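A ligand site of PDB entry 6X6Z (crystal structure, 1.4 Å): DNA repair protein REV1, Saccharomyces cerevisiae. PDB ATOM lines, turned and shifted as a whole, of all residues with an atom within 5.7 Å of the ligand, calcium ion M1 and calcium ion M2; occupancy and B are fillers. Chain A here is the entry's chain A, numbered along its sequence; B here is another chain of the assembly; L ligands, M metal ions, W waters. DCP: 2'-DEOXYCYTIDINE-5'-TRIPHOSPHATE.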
ATOM      1  N   ARG A  20     -15.182 -25.029  12.549  1.00  0.00           N
ATOM      2  CA  ARG A  20     -15.792 -24.959  11.229  1.00  0.00           C
ATOM      3  C   ARG A  20     -15.033 -24.022  10.295  1.00  0.00           C
ATOM      4  O   ARG A  20     -15.042 -24.233   9.077  1.00  0.00           O
ATOM      5  CB  ARG A  20     -17.285 -24.616  11.309  1.00  0.00           C
ATOM      6  CG  ARG A  20     -17.651 -23.159  11.031  1.00  0.00           C
ATOM      7  CD  ARG A  20     -17.562 -22.284  12.279  1.00  0.00           C
ATOM      8  NE  ARG A  20     -18.085 -20.958  11.975  1.00  0.00           N
ATOM      9  CZ  ARG A  20     -18.005 -19.904  12.777  1.00  0.00           C
ATOM     10  NH1 ARG A  20     -17.379 -19.989  13.957  1.00  0.00           N
ATOM     11  NH2 ARG A  20     -18.538 -18.746  12.406  1.00  0.00           N
ATOM     12  N   LEU A  21     -14.399 -22.988  10.836  1.00  0.00           N
ATOM     13  CA  LEU A  21     -13.615 -22.075   9.997  1.00  0.00           C
ATOM     14  C   LEU A  21     -12.373 -22.764   9.447  1.00  0.00           C
ATOM     15  O   LEU A  21     -12.009 -22.556   8.284  1.00  0.00           O
ATOM     16  CB  LEU A  21     -13.284 -20.795  10.767  1.00  0.00           C
ATOM     17  CG  LEU A  21     -14.510 -19.994  11.178  1.00  0.00           C
ATOM     18  CD1 LEU A  21     -14.074 -18.825  12.075  1.00  0.00           C
ATOM     19  CD2 LEU A  21     -15.291 -19.492   9.957  1.00  0.00           C
ATOM     20  N   LEU A  24     -13.810 -24.858   6.568  1.00  0.00           N
ATOM     21  CA  LEU A  24     -14.069 -24.046   5.378  1.00  0.00           C
ATOM     22  C   LEU A  24     -12.792 -23.823   4.580  1.00  0.00           C
ATOM     23  O   LEU A  24     -12.757 -23.997   3.358  1.00  0.00           O
ATOM     24  CB  LEU A  24     -14.692 -22.705   5.743  1.00  0.00           C
ATOM     25  CG  LEU A  24     -16.117 -22.632   6.260  1.00  0.00           C
ATOM     26  CD1 LEU A  24     -16.494 -21.166   6.473  1.00  0.00           C
ATOM     27  CD2 LEU A  24     -17.082 -23.298   5.279  1.00  0.00           C
ATOM     28  N   ASP A  58     -25.171 -21.273  -5.275  1.00  0.00           N
ATOM     29  CA  ASP A  58     -24.786 -21.320  -3.868  1.00  0.00           C
ATOM     30  C   ASP A  58     -25.898 -21.964  -3.039  1.00  0.00           C
ATOM     31  O   ASP A  58     -27.077 -21.656  -3.241  1.00  0.00           O
ATOM     32  CB  ASP A  58     -24.484 -19.882  -3.399  1.00  0.00           C
ATOM     33  CG  ASP A  58     -24.349 -19.785  -1.886  1.00  0.00           C
ATOM     34  OD1 ASP A  58     -23.208 -19.888  -1.356  1.00  0.00           O
ATOM     35  OD2 ASP A  58     -25.408 -19.608  -1.248  1.00  0.00           O
ATOM     36  N   PHE A  59     -25.514 -22.850  -2.117  1.00  0.00           N
ATOM     37  CA  PHE A  59     -26.517 -23.507  -1.262  1.00  0.00           C
ATOM     38  C   PHE A  59     -27.141 -22.486  -0.322  1.00  0.00           C
ATOM     39  O   PHE A  59     -26.434 -21.708   0.342  1.00  0.00           O
ATOM     40  CB  PHE A  59     -25.866 -24.556  -0.343  1.00  0.00           C
ATOM     41  CG  PHE A  59     -25.545 -25.899  -0.969  1.00  0.00           C
ATOM     42  CD1 PHE A  59     -24.427 -26.053  -1.766  1.00  0.00           C
ATOM     43  CD2 PHE A  59     -26.290 -27.038  -0.624  1.00  0.00           C
ATOM     44  CE1 PHE A  59     -24.076 -27.306  -2.262  1.00  0.00           C
ATOM     45  CE2 PHE A  59     -25.932 -28.288  -1.114  1.00  0.00           C
ATOM     46  CZ  PHE A  59     -24.828 -28.424  -1.936  1.00  0.00           C
ATOM     47  N   ASP A  60     -28.465 -22.528  -0.201  1.00  0.00           N
ATOM     48  CA  ASP A  60     -29.144 -21.748   0.825  1.00  0.00           C
ATOM     49  C   ASP A  60     -28.809 -22.294   2.214  1.00  0.00           C
ATOM     50  O   ASP A  60     -28.835 -23.510   2.440  1.00  0.00           O
ATOM     51  CB  ASP A  60     -30.660 -21.823   0.622  1.00  0.00           C
ATOM     52  CG  ASP A  60     -31.081 -21.319  -0.727  1.00  0.00           C
ATOM     53  OD1 ASP A  60     -30.541 -20.295  -1.148  1.00  0.00           O
ATOM     54  OD2 ASP A  60     -31.947 -21.971  -1.364  1.00  0.00           O
ATOM     55  N   CYS A  61     -28.516 -21.371   3.139  1.00  0.00           N
ATOM     56  CA  CYS A  61     -28.156 -21.661   4.534  1.00  0.00           C
ATOM     57  C   CYS A  61     -27.509 -23.034   4.687  1.00  0.00           C
ATOM     58  O   CYS A  61     -28.057 -23.925   5.339  1.00  0.00           O
ATOM     59  CB  CYS A  61     -29.346 -21.490   5.487  1.00  0.00           C
ATOM     60  SG  CYS A  61     -30.888 -22.353   5.043  1.00  0.00           S
ATOM     61  N   PHE A  62     -26.322 -23.181   4.094  1.00  0.00           N
ATOM     62  CA  PHE A  62     -25.753 -24.496   3.811  1.00  0.00           C
ATOM     63  C   PHE A  62     -25.699 -25.416   5.034  1.00  0.00           C
ATOM     64  O   PHE A  62     -26.269 -26.507   5.024  1.00  0.00           O
ATOM     65  CB  PHE A  62     -24.379 -24.323   3.167  1.00  0.00           C
ATOM     66  CG  PHE A  62     -23.667 -25.603   2.878  1.00  0.00           C
ATOM     67  CD1 PHE A  62     -24.259 -26.588   2.104  1.00  0.00           C
ATOM     68  CD2 PHE A  62     -22.381 -25.812   3.357  1.00  0.00           C
ATOM     69  CE1 PHE A  62     -23.583 -27.762   1.820  1.00  0.00           C
ATOM     70  CE2 PHE A  62     -21.705 -26.986   3.073  1.00  0.00           C
ATOM     71  CZ  PHE A  62     -22.301 -27.963   2.300  1.00  0.00           C
ATOM     72  N   PHE A  63     -24.971 -25.020   6.085  1.00  0.00           N
ATOM     73  CA  PHE A  63     -24.850 -25.915   7.234  1.00  0.00           C
ATOM     74  C   PHE A  63     -26.217 -26.187   7.870  1.00  0.00           C
ATOM     75  O   PHE A  63     -26.483 -27.295   8.321  1.00  0.00           O
ATOM     76  CB  PHE A  63     -23.935 -25.352   8.324  1.00  0.00           C
ATOM     77  CG  PHE A  63     -22.449 -25.426   8.041  1.00  0.00           C
ATOM     78  CD1 PHE A  63     -21.929 -25.776   6.795  1.00  0.00           C
ATOM     79  CD2 PHE A  63     -21.556 -25.096   9.062  1.00  0.00           C
ATOM     80  CE1 PHE A  63     -20.548 -25.781   6.584  1.00  0.00           C
ATOM     81  CE2 PHE A  63     -20.199 -25.115   8.853  1.00  0.00           C
ATOM     82  CZ  PHE A  63     -19.682 -25.457   7.623  1.00  0.00           C
ATOM     83  N   ALA A  64     -27.084 -25.168   7.938  1.00  0.00           N
ATOM     84  CA  ALA A  64     -28.400 -25.375   8.563  1.00  0.00           C
ATOM     85  C   ALA A  64     -29.209 -26.386   7.764  1.00  0.00           C
ATOM     86  O   ALA A  64     -29.843 -27.270   8.352  1.00  0.00           O
ATOM     87  CB  ALA A  64     -29.148 -24.047   8.711  1.00  0.00           C
ATOM     88  N   ILE A  96     -23.093 -18.826  15.697  1.00  0.00           N
ATOM     89  CA  ILE A  96     -24.047 -19.414  14.777  1.00  0.00           C
ATOM     90  C   ILE A  96     -23.350 -19.510  13.426  1.00  0.00           C
ATOM     91  O   ILE A  96     -23.160 -18.502  12.745  1.00  0.00           O
ATOM     92  CB  ILE A  96     -25.340 -18.586  14.691  1.00  0.00           C
ATOM     93  CG1 ILE A  96     -26.098 -18.716  16.015  1.00  0.00           C
ATOM     94  CG2 ILE A  96     -26.211 -19.017  13.502  1.00  0.00           C
ATOM     95  CD1 ILE A  96     -27.085 -17.607  16.272  1.00  0.00           C
ATOM     96  N   ALA A  97     -22.927 -20.719  13.051  1.00  0.00           N
ATOM     97  CA  ALA A  97     -22.248 -20.870  11.764  1.00  0.00           C
ATOM     98  C   ALA A  97     -23.227 -20.639  10.614  1.00  0.00           C
ATOM     99  O   ALA A  97     -22.885 -20.004   9.604  1.00  0.00           O
ATOM    100  CB  ALA A  97     -21.608 -22.243  11.667  1.00  0.00           C
ATOM    101  N   SER A  98     -24.434 -21.162  10.757  1.00  0.00           N
ATOM    102  CA  SER A  98     -25.490 -21.008   9.750  1.00  0.00           C
ATOM    103  C   SER A  98     -26.840 -20.981  10.461  1.00  0.00           C
ATOM    104  O   SER A  98     -26.989 -21.642  11.438  1.00  0.00           O
ATOM    105  CB  SER A  98     -25.416 -22.111   8.698  1.00  0.00           C
ATOM    106  OG  SER A  98     -26.365 -21.930   7.684  1.00  0.00           O
ATOM    107  N   CYS A  99     -27.738 -20.176   9.931  1.00  0.00           N
ATOM    108  CA  CYS A  99     -29.116 -20.112  10.447  1.00  0.00           C
ATOM    109  C   CYS A  99     -30.066 -20.239   9.248  1.00  0.00           C
ATOM    110  O   CYS A  99     -29.747 -19.773   8.202  1.00  0.00           O
ATOM    111  CB  CYS A  99     -29.388 -18.881  11.295  1.00  0.00           C
ATOM    112  SG  CYS A  99     -29.075 -17.307  10.466  1.00  0.00           S
ATOM    113  N   TYR A 101     -33.815 -19.623   7.177  1.00  0.00           N
ATOM    114  CA  TYR A 101     -34.493 -18.377   6.834  1.00  0.00           C
ATOM    115  C   TYR A 101     -35.610 -18.030   7.808  1.00  0.00           C
ATOM    116  O   TYR A 101     -35.954 -16.854   7.932  1.00  0.00           O
ATOM    117  CB  TYR A 101     -34.900 -18.366   5.357  1.00  0.00           C
ATOM    118  CG  TYR A 101     -33.698 -18.057   4.477  1.00  0.00           C
ATOM    119  CD1 TYR A 101     -32.736 -19.027   4.211  1.00  0.00           C
ATOM    120  CD2 TYR A 101     -33.522 -16.799   3.928  1.00  0.00           C
ATOM    121  CE1 TYR A 101     -31.614 -18.731   3.429  1.00  0.00           C
ATOM    122  CE2 TYR A 101     -32.407 -16.506   3.140  1.00  0.00           C
ATOM    123  CZ  TYR A 101     -31.464 -17.467   2.892  1.00  0.00           C
ATOM    124  OH  TYR A 101     -30.376 -17.142   2.102  1.00  0.00           O
ATOM    125  N   ARG A 104     -33.693 -16.037  10.232  1.00  0.00           N
ATOM    126  CA  ARG A 104     -33.359 -14.739   9.690  1.00  0.00           C
ATOM    127  C   ARG A 104     -34.555 -13.796   9.661  1.00  0.00           C
ATOM    128  O   ARG A 104     -34.358 -12.575   9.652  1.00  0.00           O
ATOM    129  CB  ARG A 104     -32.751 -14.889   8.292  1.00  0.00           C
ATOM    130  CG  ARG A 104     -31.467 -15.714   8.322  1.00  0.00           C
ATOM    131  CD  ARG A 104     -30.886 -15.916   6.933  1.00  0.00           C
ATOM    132  NE  ARG A 104     -29.853 -16.948   6.954  1.00  0.00           N
ATOM    133  CZ  ARG A 104     -28.942 -17.103   6.010  1.00  0.00           C
ATOM    134  NH1 ARG A 104     -28.919 -16.281   4.955  1.00  0.00           N
ATOM    135  NH2 ARG A 104     -28.043 -18.084   6.112  1.00  0.00           N
ATOM    136  N   ASN A 110     -25.807 -15.224  10.292  1.00  0.00           N
ATOM    137  CA  ASN A 110     -24.603 -16.035  10.472  1.00  0.00           C
ATOM    138  C   ASN A 110     -23.531 -15.206  11.153  1.00  0.00           C
ATOM    139  O   ASN A 110     -23.343 -14.034  10.827  1.00  0.00           O
ATOM    140  CB  ASN A 110     -24.058 -16.482   9.116  1.00  0.00           C
ATOM    141  CG  ASN A 110     -24.923 -17.517   8.425  1.00  0.00           C
ATOM    142  OD1 ASN A 110     -25.949 -17.963   8.945  1.00  0.00           O
ATOM    143  ND2 ASN A 110     -24.486 -17.911   7.232  1.00  0.00           N
ATOM    144  N   GLY A 111     -22.818 -15.818  12.091  1.00  0.00           N
ATOM    145  CA  GLY A 111     -21.759 -15.154  12.820  1.00  0.00           C
ATOM    146  C   GLY A 111     -22.177 -14.576  14.158  1.00  0.00           C
ATOM    147  O   GLY A 111     -21.313 -14.241  14.968  1.00  0.00           O
ATOM    148  N   TYR A 132     -22.980 -29.616  14.352  1.00  0.00           N
ATOM    149  CA  TYR A 132     -22.332 -29.702  13.053  1.00  0.00           C
ATOM    150  C   TYR A 132     -22.302 -31.148  12.573  1.00  0.00           C
ATOM    151  O   TYR A 132     -22.149 -32.086  13.370  1.00  0.00           O
ATOM    152  CB  TYR A 132     -20.903 -29.222  13.173  1.00  0.00           C
ATOM    153  CG  TYR A 132     -20.715 -27.758  13.505  1.00  0.00           C
ATOM    154  CD1 TYR A 132     -20.622 -27.331  14.823  1.00  0.00           C
ATOM    155  CD2 TYR A 132     -20.567 -26.816  12.502  1.00  0.00           C
ATOM    156  CE1 TYR A 132     -20.402 -25.996  15.134  1.00  0.00           C
ATOM    157  CE2 TYR A 132     -20.354 -25.472  12.800  1.00  0.00           C
ATOM    158  CZ  TYR A 132     -20.264 -25.069  14.118  1.00  0.00           C
ATOM    159  OH  TYR A 132     -20.041 -23.743  14.413  1.00  0.00           O
ATOM    160  N   SER A 161     -16.367 -21.895  -2.763  1.00  0.00           N
ATOM    161  CA  SER A 161     -16.463 -22.367  -1.394  1.00  0.00           C
ATOM    162  C   SER A 161     -16.997 -23.781  -1.430  1.00  0.00           C
ATOM    163  O   SER A 161     -17.422 -24.273  -2.479  1.00  0.00           O
ATOM    164  CB  SER A 161     -17.465 -21.507  -0.627  1.00  0.00           C
ATOM    165  OG  SER A 161     -17.215 -21.536   0.766  1.00  0.00           O
ATOM    166  N   ILE A 162     -17.004 -24.405  -0.251  1.00  0.00           N
ATOM    167  CA  ILE A 162     -17.653 -25.706  -0.082  1.00  0.00           C
ATOM    168  C   ILE A 162     -19.038 -25.745  -0.726  1.00  0.00           C
ATOM    169  O   ILE A 162     -19.444 -26.777  -1.275  1.00  0.00           O
ATOM    170  CB  ILE A 162     -17.697 -26.054   1.423  1.00  0.00           C
ATOM    171  CG1 ILE A 162     -18.223 -27.482   1.657  1.00  0.00           C
ATOM    172  CG2 ILE A 162     -18.532 -25.037   2.224  1.00  0.00           C
ATOM    173  CD1 ILE A 162     -17.216 -28.558   1.263  1.00  0.00           C
ATOM    174  N   ASP A 163     -19.768 -24.631  -0.703  1.00  0.00           N
ATOM    175  CA  ASP A 163     -21.161 -24.619  -1.106  1.00  0.00           C
ATOM    176  C   ASP A 163     -21.452 -23.678  -2.276  1.00  0.00           C
ATOM    177  O   ASP A 163     -22.621 -23.336  -2.506  1.00  0.00           O
ATOM    178  CB  ASP A 163     -22.059 -24.252   0.086  1.00  0.00           C
ATOM    179  CG  ASP A 163     -22.092 -22.761   0.339  1.00  0.00           C
ATOM    180  OD1 ASP A 163     -21.048 -22.104   0.159  1.00  0.00           O
ATOM    181  OD2 ASP A 163     -23.166 -22.242   0.729  1.00  0.00           O
ATOM    182  N   GLU A 164     -20.415 -23.277  -2.995  1.00  0.00           N
ATOM    183  CA  GLU A 164     -20.609 -22.175  -3.954  1.00  0.00           C
ATOM    184  C   GLU A 164     -19.650 -22.278  -5.138  1.00  0.00           C
ATOM    185  O   GLU A 164     -18.497 -22.497  -4.933  1.00  0.00           O
ATOM    186  CB  GLU A 164     -20.417 -20.886  -3.140  1.00  0.00           C
ATOM    187  CG  GLU A 164     -20.652 -19.558  -3.841  1.00  0.00           C
ATOM    188  CD  GLU A 164     -20.464 -18.426  -2.850  1.00  0.00           C
ATOM    189  OE1 GLU A 164     -20.565 -17.267  -3.318  1.00  0.00           O
ATOM    190  OE2 GLU A 164     -20.266 -18.667  -1.613  1.00  0.00           O
ATOM    191  N   LYS A 221     -32.382 -15.300  -3.271  1.00  0.00           N
ATOM    192  CA  LYS A 221     -32.506 -16.149  -2.101  1.00  0.00           C
ATOM    193  C   LYS A 221     -33.766 -15.820  -1.307  1.00  0.00           C
ATOM    194  O   LYS A 221     -34.232 -14.671  -1.302  1.00  0.00           O
ATOM    195  CB  LYS A 221     -31.287 -15.999  -1.208  1.00  0.00           C
ATOM    196  CG  LYS A 221     -30.098 -16.777  -1.749  1.00  0.00           C
ATOM    197  CD  LYS A 221     -28.856 -16.530  -0.946  1.00  0.00           C
ATOM    198  CE  LYS A 221     -27.752 -17.503  -1.357  1.00  0.00           C
ATOM    199  NZ  LYS A 221     -27.993 -18.871  -0.776  1.00  0.00           N
ATOM    200  P    DG B  12     -16.233 -15.356  -1.060  1.00  0.00           P
ATOM    201  OP1  DG B  12     -15.102 -15.574  -1.920  1.00  0.00           O
ATOM    202  OP2  DG B  12     -17.349 -14.568  -1.441  1.00  0.00           O
ATOM    203  O5'  DG B  12     -16.772 -16.795  -0.645  1.00  0.00           O
ATOM    204  C5'  DG B  12     -17.944 -16.909   0.121  1.00  0.00           C
ATOM    205  C4'  DG B  12     -17.667 -17.896   1.233  1.00  0.00           C
ATOM    206  O4'  DG B  12     -16.835 -17.257   2.205  1.00  0.00           O
ATOM    207  C3'  DG B  12     -18.894 -18.321   2.023  1.00  0.00           C
ATOM    208  O3'  DG B  12     -19.310 -19.578   1.548  1.00  0.00           O
ATOM    209  C2'  DG B  12     -18.325 -18.652   3.390  1.00  0.00           C
ATOM    210  C1'  DG B  12     -16.942 -17.993   3.379  1.00  0.00           C
ATOM    211  N9   DG B  12     -16.664 -17.119   4.489  1.00  0.00           N
ATOM    212  C8   DG B  12     -17.471 -16.180   5.073  1.00  0.00           C
ATOM    213  N7   DG B  12     -16.924 -15.592   6.094  1.00  0.00           N
ATOM    214  C5   DG B  12     -15.655 -16.155   6.172  1.00  0.00           C
ATOM    215  C6   DG B  12     -14.596 -15.935   7.087  1.00  0.00           C
ATOM    216  O6   DG B  12     -14.554 -15.168   8.042  1.00  0.00           O
ATOM    217  N1   DG B  12     -13.501 -16.725   6.805  1.00  0.00           N
ATOM    218  C2   DG B  12     -13.433 -17.627   5.774  1.00  0.00           C
ATOM    219  N2   DG B  12     -12.304 -18.322   5.679  1.00  0.00           N
ATOM    220  N3   DG B  12     -14.411 -17.858   4.931  1.00  0.00           N
ATOM    221  C4   DG B  12     -15.483 -17.098   5.186  1.00  0.00           C
HETATM  222  N1  DCP L   1     -20.121 -20.042   7.637  1.00  0.00           N
HETATM  223  C2  DCP L   1     -19.650 -19.957   9.024  1.00  0.00           C
HETATM  224  N3  DCP L   1     -19.550 -18.634   9.654  1.00  0.00           N
HETATM  225  C4  DCP L   1     -19.919 -17.467   8.913  1.00  0.00           C
HETATM  226  C5  DCP L   1     -20.385 -17.548   7.518  1.00  0.00           C
HETATM  227  C6  DCP L   1     -20.475 -18.863   6.873  1.00  0.00           C
HETATM  228  O2  DCP L   1     -19.372 -20.950   9.575  1.00  0.00           O
HETATM  229  N4  DCP L   1     -19.821 -16.193   9.554  1.00  0.00           N
HETATM  230  C1' DCP L   1     -20.219 -21.372   7.135  1.00  0.00           C
HETATM  231  C2' DCP L   1     -21.447 -21.884   7.360  1.00  0.00           C
HETATM  232  C3' DCP L   1     -22.291 -21.539   6.031  1.00  0.00           C
HETATM  233  C4' DCP L   1     -21.377 -21.798   5.023  1.00  0.00           C
HETATM  234  O4' DCP L   1     -20.064 -21.267   5.589  1.00  0.00           O
HETATM  235  O3' DCP L   1     -23.489 -22.331   5.925  1.00  0.00           O
HETATM  236  C5' DCP L   1     -21.593 -21.026   3.723  1.00  0.00           C
HETATM  237  O5' DCP L   1     -21.530 -19.638   3.947  1.00  0.00           O
HETATM  238  PA  DCP L   1     -22.559 -18.659   3.162  1.00  0.00           P
HETATM  239  O1A DCP L   1     -22.045 -17.260   3.294  1.00  0.00           O
HETATM  240  O2A DCP L   1     -22.836 -19.154   1.768  1.00  0.00           O
HETATM  241  O3A DCP L   1     -23.919 -18.690   4.057  1.00  0.00           O
HETATM  242  PB  DCP L   1     -25.128 -19.768   4.121  1.00  0.00           P
HETATM  243  O1B DCP L   1     -25.259 -20.255   5.537  1.00  0.00           O
HETATM  244  O2B DCP L   1     -25.007 -20.809   3.065  1.00  0.00           O
HETATM  245  O3B DCP L   1     -26.461 -18.865   3.853  1.00  0.00           O
HETATM  246  PG  DCP L   1     -26.854 -18.075   2.474  1.00  0.00           P
HETATM  247  O1G DCP L   1     -28.211 -18.635   2.086  1.00  0.00           O
HETATM  248  O2G DCP L   1     -26.928 -16.615   2.854  1.00  0.00           O
HETATM  249  O3G DCP L   1     -25.806 -18.384   1.449  1.00  0.00           O
HETATM  250 CA    CA M   1     -21.336 -19.726   0.030  1.00  0.00          CA
HETATM  251 CA    CA M   2     -24.578 -20.387   0.823  1.00  0.00          CA
HETATM  252  O   HOH W   1     -25.464 -15.326   4.829  1.00  0.00           O
HETATM  253  O   HOH W   2     -20.330 -13.716   8.204  1.00  0.00           O
HETATM  254  O   HOH W   3     -22.857 -16.011   5.606  1.00  0.00           O
HETATM  255  O   HOH W   4     -27.114 -14.354   1.380  1.00  0.00           O
HETATM  256  O   HOH W   5     -24.462 -16.445  -0.044  1.00  0.00           O
HETATM  257  O   HOH W   6     -21.732 -16.780  -0.045  1.00  0.00           O
HETATM  258  O   HOH W   7     -23.516 -15.045   2.108  1.00  0.00           O
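Of the 25 residues printed, 3 come within 4 Å of calcium ion M2. The nearest printed residue that does not touch calcium ion M2 is Lys 221 (4.1 Å).
An oxygen (O2B) of the ligand is bound to calcium ion M2. O of Phe 59 is bound to calcium ion M2 (2.3 Å). Calcium ion M2 is bound by OD2 of Asp 163. O2A of the ligand binds calcium ion M2 (2.3 Å). OD2 of Asp 58 is bound to calcium ion M2 (2.4 Å). Calcium ion M2 is bound by an oxygen (O3G) of the ligand, 2.4 Å away. OD1 of Asp 58 binds calcium ion M2, at 2.6 Å.
The side-chain hydroxyl (OH) of Tyr 101 lies within hydrogen-bond range of an oxygen (O1G) of the ligand (2.6 Å). O2 of the ligand is in hydrogen-bond range of NE of Arg 20, at 2.7 Å. The guanidinium group (NH1) of Arg 104 lies within salt-bridge range of an oxygen (O2G) of the ligand. The side-chain amino group of Lys 221 is in salt-bridge range of an oxygen (O1G) of the ligand. The backbone NH (N) of Phe 62 sits at hydrogen-bond distance from an oxygen (O1B) of the ligand. The side-chain hydroxyl (OG) of Ser 98 sits at hydrogen-bond distance from an oxygen (O1B) of the ligand. An oxygen (O1G) of the ligand sits at hydrogen-bond distance from the backbone NH (N) of Cys 61 (2.9 Å). An oxygen (O1B) of the ligand is in hydrogen-bond range of the side-chain amide nitrogen of Asn 110, 3.0 Å away. O3' of the ligand lies within hydrogen-bond range of N of Phe 63.
N1 of the ligand lies close to O of Ala 97, 3.4 Å away. Leu 24 touches the ligand. Asp 60 touches the ligand. CA of Gly 111 touches N4 of the ligand, 3.9 Å away. Within 4 Å of the ligand: Arg 20, Leu 24, Asp 58, Phe 59, Asp 60, Cys 61, Phe 62, Phe 63, Ala 97, Ser 98, Tyr 101, Arg 104, Asn 110, Gly 111, Asp 163, Lys 221 and DG 12 of chain B. The nearest printed residue that does not touch the ligand is Glu 164 (4.3 Å).
Calcium ion M1 is bound by the side-chain carboxylate of Glu 164 (2.2 Å), the side-chain carboxylate of Asp 58 (2.3 Å), an oxygen (O2A) of the ligand (2.4 Å), the side-chain carboxylate of Asp 163 (2.4 Å) and O3' of DG 12 of chain B (2.5 Å). Calcium ion M1 has five donor atoms within binding distance. Slightly farther from calcium ion M1 lies water W6 (3.0 Å).
O of Phe 59 sits close to NZ of Lys 221 (3.4 Å). OD2 of Asp 58 lies close to NZ of Lys 221 (2.7 Å). The side-chain hydroxyl (OG) of Ser 161 sits close to O3' of DG 12 of chain B, at 3.0 Å. The guanidinium group (NE) of Arg 104 lies within hydrogen-bond range of the backbone carbonyl oxygen (O) of Cys 99 (3.1 Å). The side-chain carboxylate (OD1) of Asp 60 lies within salt-bridge range of the side-chain amino group (NZ) of Lys 221 (2.9 Å). The backbone NH (N) of Ala 64 lies within hydrogen-bond range of the side-chain hydroxyl (OG) of Ser 98, at 3.3 Å. The side-chain amide oxygen (OD1) of Asn 110 is in hydrogen-bond range of the backbone NH (N) of Cys 99, 3.0 Å away. The backbone carbonyl oxygen of Ile 96 is in hydrogen-bond range of the backbone NH of Gly 111 (2.8 Å).
Water W3 bridges O1A of the ligand (2.8 Å) and ND2 of Asn 110 (3.0 Å).
Within 4 Å of calcium ion M1: Asp 58, Asp 163, Glu 164 and DG 12 of chain B.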
